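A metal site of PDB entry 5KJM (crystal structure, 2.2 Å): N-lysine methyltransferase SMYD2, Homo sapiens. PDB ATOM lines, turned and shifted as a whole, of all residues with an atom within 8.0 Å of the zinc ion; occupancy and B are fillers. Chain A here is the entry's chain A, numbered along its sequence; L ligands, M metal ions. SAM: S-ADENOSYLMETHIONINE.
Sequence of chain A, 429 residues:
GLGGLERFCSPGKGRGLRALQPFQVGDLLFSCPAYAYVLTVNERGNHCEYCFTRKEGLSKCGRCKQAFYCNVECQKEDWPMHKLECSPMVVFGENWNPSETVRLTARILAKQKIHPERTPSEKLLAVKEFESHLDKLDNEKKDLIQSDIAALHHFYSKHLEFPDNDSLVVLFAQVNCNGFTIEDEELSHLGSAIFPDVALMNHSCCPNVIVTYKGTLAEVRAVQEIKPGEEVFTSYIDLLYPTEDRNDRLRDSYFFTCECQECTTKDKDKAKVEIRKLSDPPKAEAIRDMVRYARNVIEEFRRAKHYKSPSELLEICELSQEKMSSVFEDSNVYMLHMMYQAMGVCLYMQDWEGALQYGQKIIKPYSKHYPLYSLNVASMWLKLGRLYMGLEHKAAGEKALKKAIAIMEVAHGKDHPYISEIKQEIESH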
ATOM      1  N   HIS A 203      31.165   7.390 -15.653  1.00  0.00           N
ATOM      2  CA  HIS A 203      30.085   6.525 -16.118  1.00  0.00           C
ATOM      3  C   HIS A 203      29.635   5.463 -15.147  1.00  0.00           C
ATOM      4  O   HIS A 203      30.453   4.845 -14.449  1.00  0.00           O
ATOM      5  CB  HIS A 203      30.467   5.822 -17.431  1.00  0.00           C
ATOM      6  CG  HIS A 203      29.433   4.837 -17.884  1.00  0.00           C
ATOM      7  ND1 HIS A 203      29.506   3.489 -17.526  1.00  0.00           N
ATOM      8  CD2 HIS A 203      28.295   5.034 -18.587  1.00  0.00           C
ATOM      9  CE1 HIS A 203      28.432   2.931 -18.044  1.00  0.00           C
ATOM     10  NE2 HIS A 203      27.682   3.815 -18.678  1.00  0.00           N
ATOM     11  N   SER A 204      28.338   5.162 -15.194  1.00  0.00           N
ATOM     12  CA  SER A 204      27.713   4.032 -14.539  1.00  0.00           C
ATOM     13  C   SER A 204      26.549   3.545 -15.371  1.00  0.00           C
ATOM     14  O   SER A 204      25.844   4.366 -15.964  1.00  0.00           O
ATOM     15  CB  SER A 204      27.240   4.361 -13.126  1.00  0.00           C
ATOM     16  OG  SER A 204      26.669   3.192 -12.574  1.00  0.00           O
ATOM     17  N   CYS A 205      26.316   2.225 -15.393  1.00  0.00           N
ATOM     18  CA  CYS A 205      25.160   1.637 -16.061  1.00  0.00           C
ATOM     19  C   CYS A 205      23.919   1.732 -15.193  1.00  0.00           C
ATOM     20  O   CYS A 205      22.827   1.502 -15.693  1.00  0.00           O
ATOM     21  CB  CYS A 205      25.426   0.218 -16.549  1.00  0.00           C
ATOM     22  SG  CYS A 205      26.820   0.086 -17.685  1.00  0.00           S
ATOM     23  N   CYS A 206      24.077   2.101 -13.907  1.00  0.00           N
ATOM     24  CA  CYS A 206      22.976   2.457 -13.011  1.00  0.00           C
ATOM     25  C   CYS A 206      23.269   3.871 -12.537  1.00  0.00           C
ATOM     26  O   CYS A 206      23.753   4.066 -11.425  1.00  0.00           O
ATOM     27  CB  CYS A 206      22.757   1.477 -11.854  1.00  0.00           C
ATOM     28  SG  CYS A 206      24.203   0.510 -11.386  1.00  0.00           S
ATOM     29  N   ILE A 237      26.243   5.754 -22.414  1.00  0.00           N
ATOM     30  CA  ILE A 237      25.725   4.945 -23.517  1.00  0.00           C
ATOM     31  C   ILE A 237      24.252   4.560 -23.344  1.00  0.00           C
ATOM     32  O   ILE A 237      23.644   4.808 -22.292  1.00  0.00           O
ATOM     33  CB  ILE A 237      26.615   3.644 -23.581  1.00  0.00           C
ATOM     34  CG1 ILE A 237      26.721   2.975 -22.168  1.00  0.00           C
ATOM     35  CG2 ILE A 237      28.038   3.952 -24.168  1.00  0.00           C
ATOM     36  CD1 ILE A 237      26.986   1.520 -22.152  1.00  0.00           C
ATOM     37  N   LEU A 239      21.580   2.100 -22.490  1.00  0.00           N
ATOM     38  CA  LEU A 239      21.486   1.054 -21.470  1.00  0.00           C
ATOM     39  C   LEU A 239      20.538  -0.102 -21.794  1.00  0.00           C
ATOM     40  O   LEU A 239      20.311  -0.957 -20.930  1.00  0.00           O
ATOM     41  CB  LEU A 239      21.099   1.698 -20.119  1.00  0.00           C
ATOM     42  CG  LEU A 239      22.083   2.721 -19.554  1.00  0.00           C
ATOM     43  CD1 LEU A 239      21.561   3.338 -18.290  1.00  0.00           C
ATOM     44  CD2 LEU A 239      23.469   2.114 -19.343  1.00  0.00           C
ATOM     45  N   THR A 243      25.440  -6.599 -20.839  1.00  0.00           N
ATOM     46  CA  THR A 243      26.734  -6.205 -20.263  1.00  0.00           C
ATOM     47  C   THR A 243      27.885  -6.209 -21.296  1.00  0.00           C
ATOM     48  O   THR A 243      28.560  -5.190 -21.439  1.00  0.00           O
ATOM     49  CB  THR A 243      27.012  -7.074 -19.018  1.00  0.00           C
ATOM     50  OG1 THR A 243      25.969  -6.808 -18.063  1.00  0.00           O
ATOM     51  CG2 THR A 243      28.385  -6.823 -18.398  1.00  0.00           C
ATOM     52  N   ARG A 246      27.537  -3.377 -23.858  1.00  0.00           N
ATOM     53  CA  ARG A 246      27.755  -2.076 -23.220  1.00  0.00           C
ATOM     54  C   ARG A 246      29.261  -1.789 -23.079  1.00  0.00           C
ATOM     55  O   ARG A 246      29.750  -0.734 -23.487  1.00  0.00           O
ATOM     56  CB  ARG A 246      27.059  -2.032 -21.845  1.00  0.00           C
ATOM     57  CG  ARG A 246      25.525  -1.970 -21.924  1.00  0.00           C
ATOM     58  CD  ARG A 246      24.859  -1.507 -20.618  1.00  0.00           C
ATOM     59  NE  ARG A 246      25.402  -2.133 -19.391  1.00  0.00           N
ATOM     60  CZ  ARG A 246      25.011  -3.306 -18.894  1.00  0.00           C
ATOM     61  NH1 ARG A 246      24.107  -4.036 -19.528  1.00  0.00           N
ATOM     62  NH2 ARG A 246      25.552  -3.771 -17.783  1.00  0.00           N
ATOM     63  N   ASN A 247      30.001  -2.783 -22.552  1.00  0.00           N
ATOM     64  CA  ASN A 247      31.436  -2.715 -22.317  1.00  0.00           C
ATOM     65  C   ASN A 247      32.263  -2.740 -23.602  1.00  0.00           C
ATOM     66  O   ASN A 247      33.350  -2.164 -23.624  1.00  0.00           O
ATOM     67  CB  ASN A 247      31.893  -3.775 -21.318  1.00  0.00           C
ATOM     68  CG  ASN A 247      31.608  -3.320 -19.907  1.00  0.00           C
ATOM     69  OD1 ASN A 247      32.068  -2.261 -19.482  1.00  0.00           O
ATOM     70  ND2 ASN A 247      30.720  -4.008 -19.226  1.00  0.00           N
ATOM     71  N   LEU A 250      31.839   0.869 -24.530  1.00  0.00           N
ATOM     72  CA  LEU A 250      32.605   1.667 -23.572  1.00  0.00           C
ATOM     73  C   LEU A 250      34.094   1.565 -23.816  1.00  0.00           C
ATOM     74  O   LEU A 250      34.761   2.593 -23.775  1.00  0.00           O
ATOM     75  CB  LEU A 250      32.261   1.293 -22.118  1.00  0.00           C
ATOM     76  CG  LEU A 250      30.895   1.743 -21.622  1.00  0.00           C
ATOM     77  CD1 LEU A 250      30.583   1.124 -20.282  1.00  0.00           C
ATOM     78  CD2 LEU A 250      30.766   3.291 -21.609  1.00  0.00           C
ATOM     79  N   PHE A 256      37.578   2.208 -21.533  1.00  0.00           N
ATOM     80  CA  PHE A 256      37.500   1.631 -20.186  1.00  0.00           C
ATOM     81  C   PHE A 256      36.445   0.534 -20.111  1.00  0.00           C
ATOM     82  O   PHE A 256      35.522   0.510 -20.922  1.00  0.00           O
ATOM     83  CB  PHE A 256      37.232   2.724 -19.121  1.00  0.00           C
ATOM     84  CG  PHE A 256      35.790   3.185 -19.035  1.00  0.00           C
ATOM     85  CD1 PHE A 256      34.905   2.567 -18.146  1.00  0.00           C
ATOM     86  CD2 PHE A 256      35.316   4.216 -19.833  1.00  0.00           C
ATOM     87  CE1 PHE A 256      33.567   2.971 -18.084  1.00  0.00           C
ATOM     88  CE2 PHE A 256      33.978   4.627 -19.750  1.00  0.00           C
ATOM     89  CZ  PHE A 256      33.109   4.006 -18.878  1.00  0.00           C
ATOM     90  N   THR A 257      36.559  -0.324 -19.084  1.00  0.00           N
ATOM     91  CA  THR A 257      35.569  -1.338 -18.793  1.00  0.00           C
ATOM     92  C   THR A 257      34.868  -0.904 -17.494  1.00  0.00           C
ATOM     93  O   THR A 257      35.536  -0.546 -16.514  1.00  0.00           O
ATOM     94  CB  THR A 257      36.204  -2.724 -18.683  1.00  0.00           C
ATOM     95  OG1 THR A 257      36.850  -3.019 -19.906  1.00  0.00           O
ATOM     96  CG2 THR A 257      35.178  -3.826 -18.351  1.00  0.00           C
ATOM     97  N   CYS A 258      33.537  -0.909 -17.505  1.00  0.00           N
ATOM     98  CA  CYS A 258      32.697  -0.560 -16.374  1.00  0.00           C
ATOM     99  C   CYS A 258      32.650  -1.704 -15.386  1.00  0.00           C
ATOM    100  O   CYS A 258      32.599  -2.872 -15.795  1.00  0.00           O
ATOM    101  CB  CYS A 258      31.291  -0.184 -16.850  1.00  0.00           C
ATOM    102  SG  CYS A 258      30.223   0.484 -15.549  1.00  0.00           S
ATOM    103  N   GLU A 259      32.605  -1.377 -14.088  1.00  0.00           N
ATOM    104  CA  GLU A 259      32.507  -2.352 -12.997  1.00  0.00           C
ATOM    105  C   GLU A 259      31.348  -2.009 -12.057  1.00  0.00           C
ATOM    106  O   GLU A 259      31.383  -2.380 -10.883  1.00  0.00           O
ATOM    107  CB  GLU A 259      33.816  -2.413 -12.173  1.00  0.00           C
ATOM    108  CG  GLU A 259      35.036  -2.942 -12.877  1.00  0.00           C
ATOM    109  CD  GLU A 259      36.176  -3.156 -11.896  1.00  0.00           C
ATOM    110  OE1 GLU A 259      36.223  -4.232 -11.269  1.00  0.00           O
ATOM    111  OE2 GLU A 259      36.970  -2.204 -11.684  1.00  0.00           O
ATOM    112  N   CYS A 260      30.339  -1.304 -12.562  1.00  0.00           N
ATOM    113  CA  CYS A 260      29.153  -0.943 -11.785  1.00  0.00           C
ATOM    114  C   CYS A 260      28.331  -2.184 -11.381  1.00  0.00           C
ATOM    115  O   CYS A 260      28.572  -3.275 -11.913  1.00  0.00           O
ATOM    116  CB  CYS A 260      28.295   0.072 -12.526  1.00  0.00           C
ATOM    117  SG  CYS A 260      27.151  -0.651 -13.724  1.00  0.00           S
ATOM    118  N   GLN A 261      27.348  -2.013 -10.464  1.00  0.00           N
ATOM    119  CA  GLN A 261      26.544  -3.136  -9.989  1.00  0.00           C
ATOM    120  C   GLN A 261      25.932  -3.921 -11.122  1.00  0.00           C
ATOM    121  O   GLN A 261      25.994  -5.151 -11.088  1.00  0.00           O
ATOM    122  CB  GLN A 261      25.488  -2.707  -8.954  1.00  0.00           C
ATOM    123  CG  GLN A 261      25.087  -3.839  -7.997  1.00  0.00           C
ATOM    124  CD  GLN A 261      26.200  -4.167  -7.009  1.00  0.00           C
ATOM    125  OE1 GLN A 261      26.408  -3.465  -6.009  1.00  0.00           O
ATOM    126  NE2 GLN A 261      26.958  -5.233  -7.285  1.00  0.00           N
ATOM    127  N   GLU A 262      25.406  -3.244 -12.135  1.00  0.00           N
ATOM    128  CA  GLU A 262      24.813  -3.895 -13.306  1.00  0.00           C
ATOM    129  C   GLU A 262      25.802  -4.781 -14.106  1.00  0.00           C
ATOM    130  O   GLU A 262      25.433  -5.879 -14.519  1.00  0.00           O
ATOM    131  CB  GLU A 262      24.113  -2.866 -14.213  1.00  0.00           C
ATOM    132  CG  GLU A 262      23.199  -3.492 -15.256  1.00  0.00           C
ATOM    133  CD  GLU A 262      22.212  -4.516 -14.741  1.00  0.00           C
ATOM    134  OE1 GLU A 262      22.268  -5.683 -15.211  1.00  0.00           O
ATOM    135  OE2 GLU A 262      21.386  -4.175 -13.860  1.00  0.00           O
ATOM    136  N   CYS A 263      27.032  -4.295 -14.312  1.00  0.00           N
ATOM    137  CA  CYS A 263      28.043  -5.040 -15.076  1.00  0.00           C
ATOM    138  C   CYS A 263      28.627  -6.215 -14.255  1.00  0.00           C
ATOM    139  O   CYS A 263      28.952  -7.259 -14.821  1.00  0.00           O
ATOM    140  CB  CYS A 263      29.124  -4.104 -15.620  1.00  0.00           C
ATOM    141  SG  CYS A 263      28.500  -2.811 -16.743  1.00  0.00           S
ATOM    142  N   THR A 264      28.683  -6.056 -12.909  1.00  0.00           N
ATOM    143  CA  THR A 264      29.202  -7.065 -11.979  1.00  0.00           C
ATOM    144  C   THR A 264      28.173  -8.195 -11.794  1.00  0.00           C
ATOM    145  O   THR A 264      28.492  -9.383 -11.953  1.00  0.00           O
ATOM    146  CB  THR A 264      29.634  -6.393 -10.654  1.00  0.00           C
ATOM    147  OG1 THR A 264      30.670  -5.449 -10.925  1.00  0.00           O
ATOM    148  CG2 THR A 264      30.148  -7.383  -9.627  1.00  0.00           C
HETATM  149  N   SAM L   1      37.472  10.605 -15.281  1.00  0.00           N
HETATM  150  CA  SAM L   1      37.516  11.648 -16.335  1.00  0.00           C
HETATM  151  C   SAM L   1      38.697  12.674 -16.142  1.00  0.00           C
HETATM  152  O   SAM L   1      38.836  13.568 -17.008  1.00  0.00           O
HETATM  153  OXT SAM L   1      39.438  12.527 -15.135  1.00  0.00           O
HETATM  154  CB  SAM L   1      36.136  12.370 -16.384  1.00  0.00           C
HETATM  155  CG  SAM L   1      35.214  11.647 -17.365  1.00  0.00           C
HETATM  156  SD  SAM L   1      35.829  11.714 -19.070  1.00  0.00           S
HETATM  157  CE  SAM L   1      34.510  12.452 -19.901  1.00  0.00           C
HETATM  158  C5' SAM L   1      35.628   9.988 -19.601  1.00  0.00           C
HETATM  159  C4' SAM L   1      36.796   9.086 -19.195  1.00  0.00           C
HETATM  160  O4' SAM L   1      36.737   8.830 -17.779  1.00  0.00           O
HETATM  161  C3' SAM L   1      36.786   7.705 -19.840  1.00  0.00           C
HETATM  162  O3' SAM L   1      37.336   7.745 -21.145  1.00  0.00           O
HETATM  163  C2' SAM L   1      37.538   6.860 -18.814  1.00  0.00           C
HETATM  164  O2' SAM L   1      38.963   6.915 -18.895  1.00  0.00           O
HETATM  165  C1' SAM L   1      37.074   7.481 -17.497  1.00  0.00           C
HETATM  166  N9  SAM L   1      35.933   6.806 -16.884  1.00  0.00           N
HETATM  167  C8  SAM L   1      34.629   7.239 -16.857  1.00  0.00           C
HETATM  168  N7  SAM L   1      33.805   6.436 -16.235  1.00  0.00           N
HETATM  169  C5  SAM L   1      34.615   5.393 -15.816  1.00  0.00           C
HETATM  170  C6  SAM L   1      34.362   4.217 -15.082  1.00  0.00           C
HETATM  171  N6  SAM L   1      33.158   3.892 -14.596  1.00  0.00           N
HETATM  172  N1  SAM L   1      35.392   3.375 -14.842  1.00  0.00           N
HETATM  173  C2  SAM L   1      36.607   3.710 -15.312  1.00  0.00           C
HETATM  174  N3  SAM L   1      36.981   4.788 -16.010  1.00  0.00           N
HETATM  175  C4  SAM L   1      35.929   5.603 -16.219  1.00  0.00           C
HETATM  176 ZN    ZN M   1      28.279  -0.781 -15.915  1.00  0.00          ZN
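N7 of the ligand is in hydrogen-bond range of N of His 203.
The backbone carbonyl oxygen (O) of His 203 lies within hydrogen-bond range of a nitrogen (N6) of the ligand, at 2.9 Å.
The side-chain sulfur (SG) of Cys 263 sits close to the guanidinium group (NH2) of Arg 246, at 3.3 Å.
SG of Cys 263 lies close to ND2 of Asn 247, 3.5 Å away.
SG of Cys 258 sits close to ND1 of His 203 (3.7 Å).
The backbone NH of Cys 258 sits at hydrogen-bond distance from the side-chain amide oxygen of Asn 247 (2.8 Å).
The guanidinium group (NE) of Arg 246 lies close to the side-chain sulfur (SG) of Cys 205 (3.1 Å).
The side-chain sulfur (SG) of Cys 260 lies close to the backbone NH (N) of Glu 262 (3.5 Å).
OG1 of Thr 264 sits at hydrogen-bond distance from O of Cys 260.
Of the 19 residues printed, 4 come within 4 Å of the zinc ion.
Along chain A the residues within 4 Å of the zinc ion span positions 205 to 263.
The nearest printed residue that does not touch the zinc ion is His 203 (4.3 Å).
The zinc ion is bound by the side-chain sulfur of Cys 263 (2.2 Å), the side-chain sulfur of Cys 258 (2.3 Å), the side-chain sulfur of Cys 205 (2.5 Å) and the side-chain sulfur of Cys 260 (2.5 Å).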
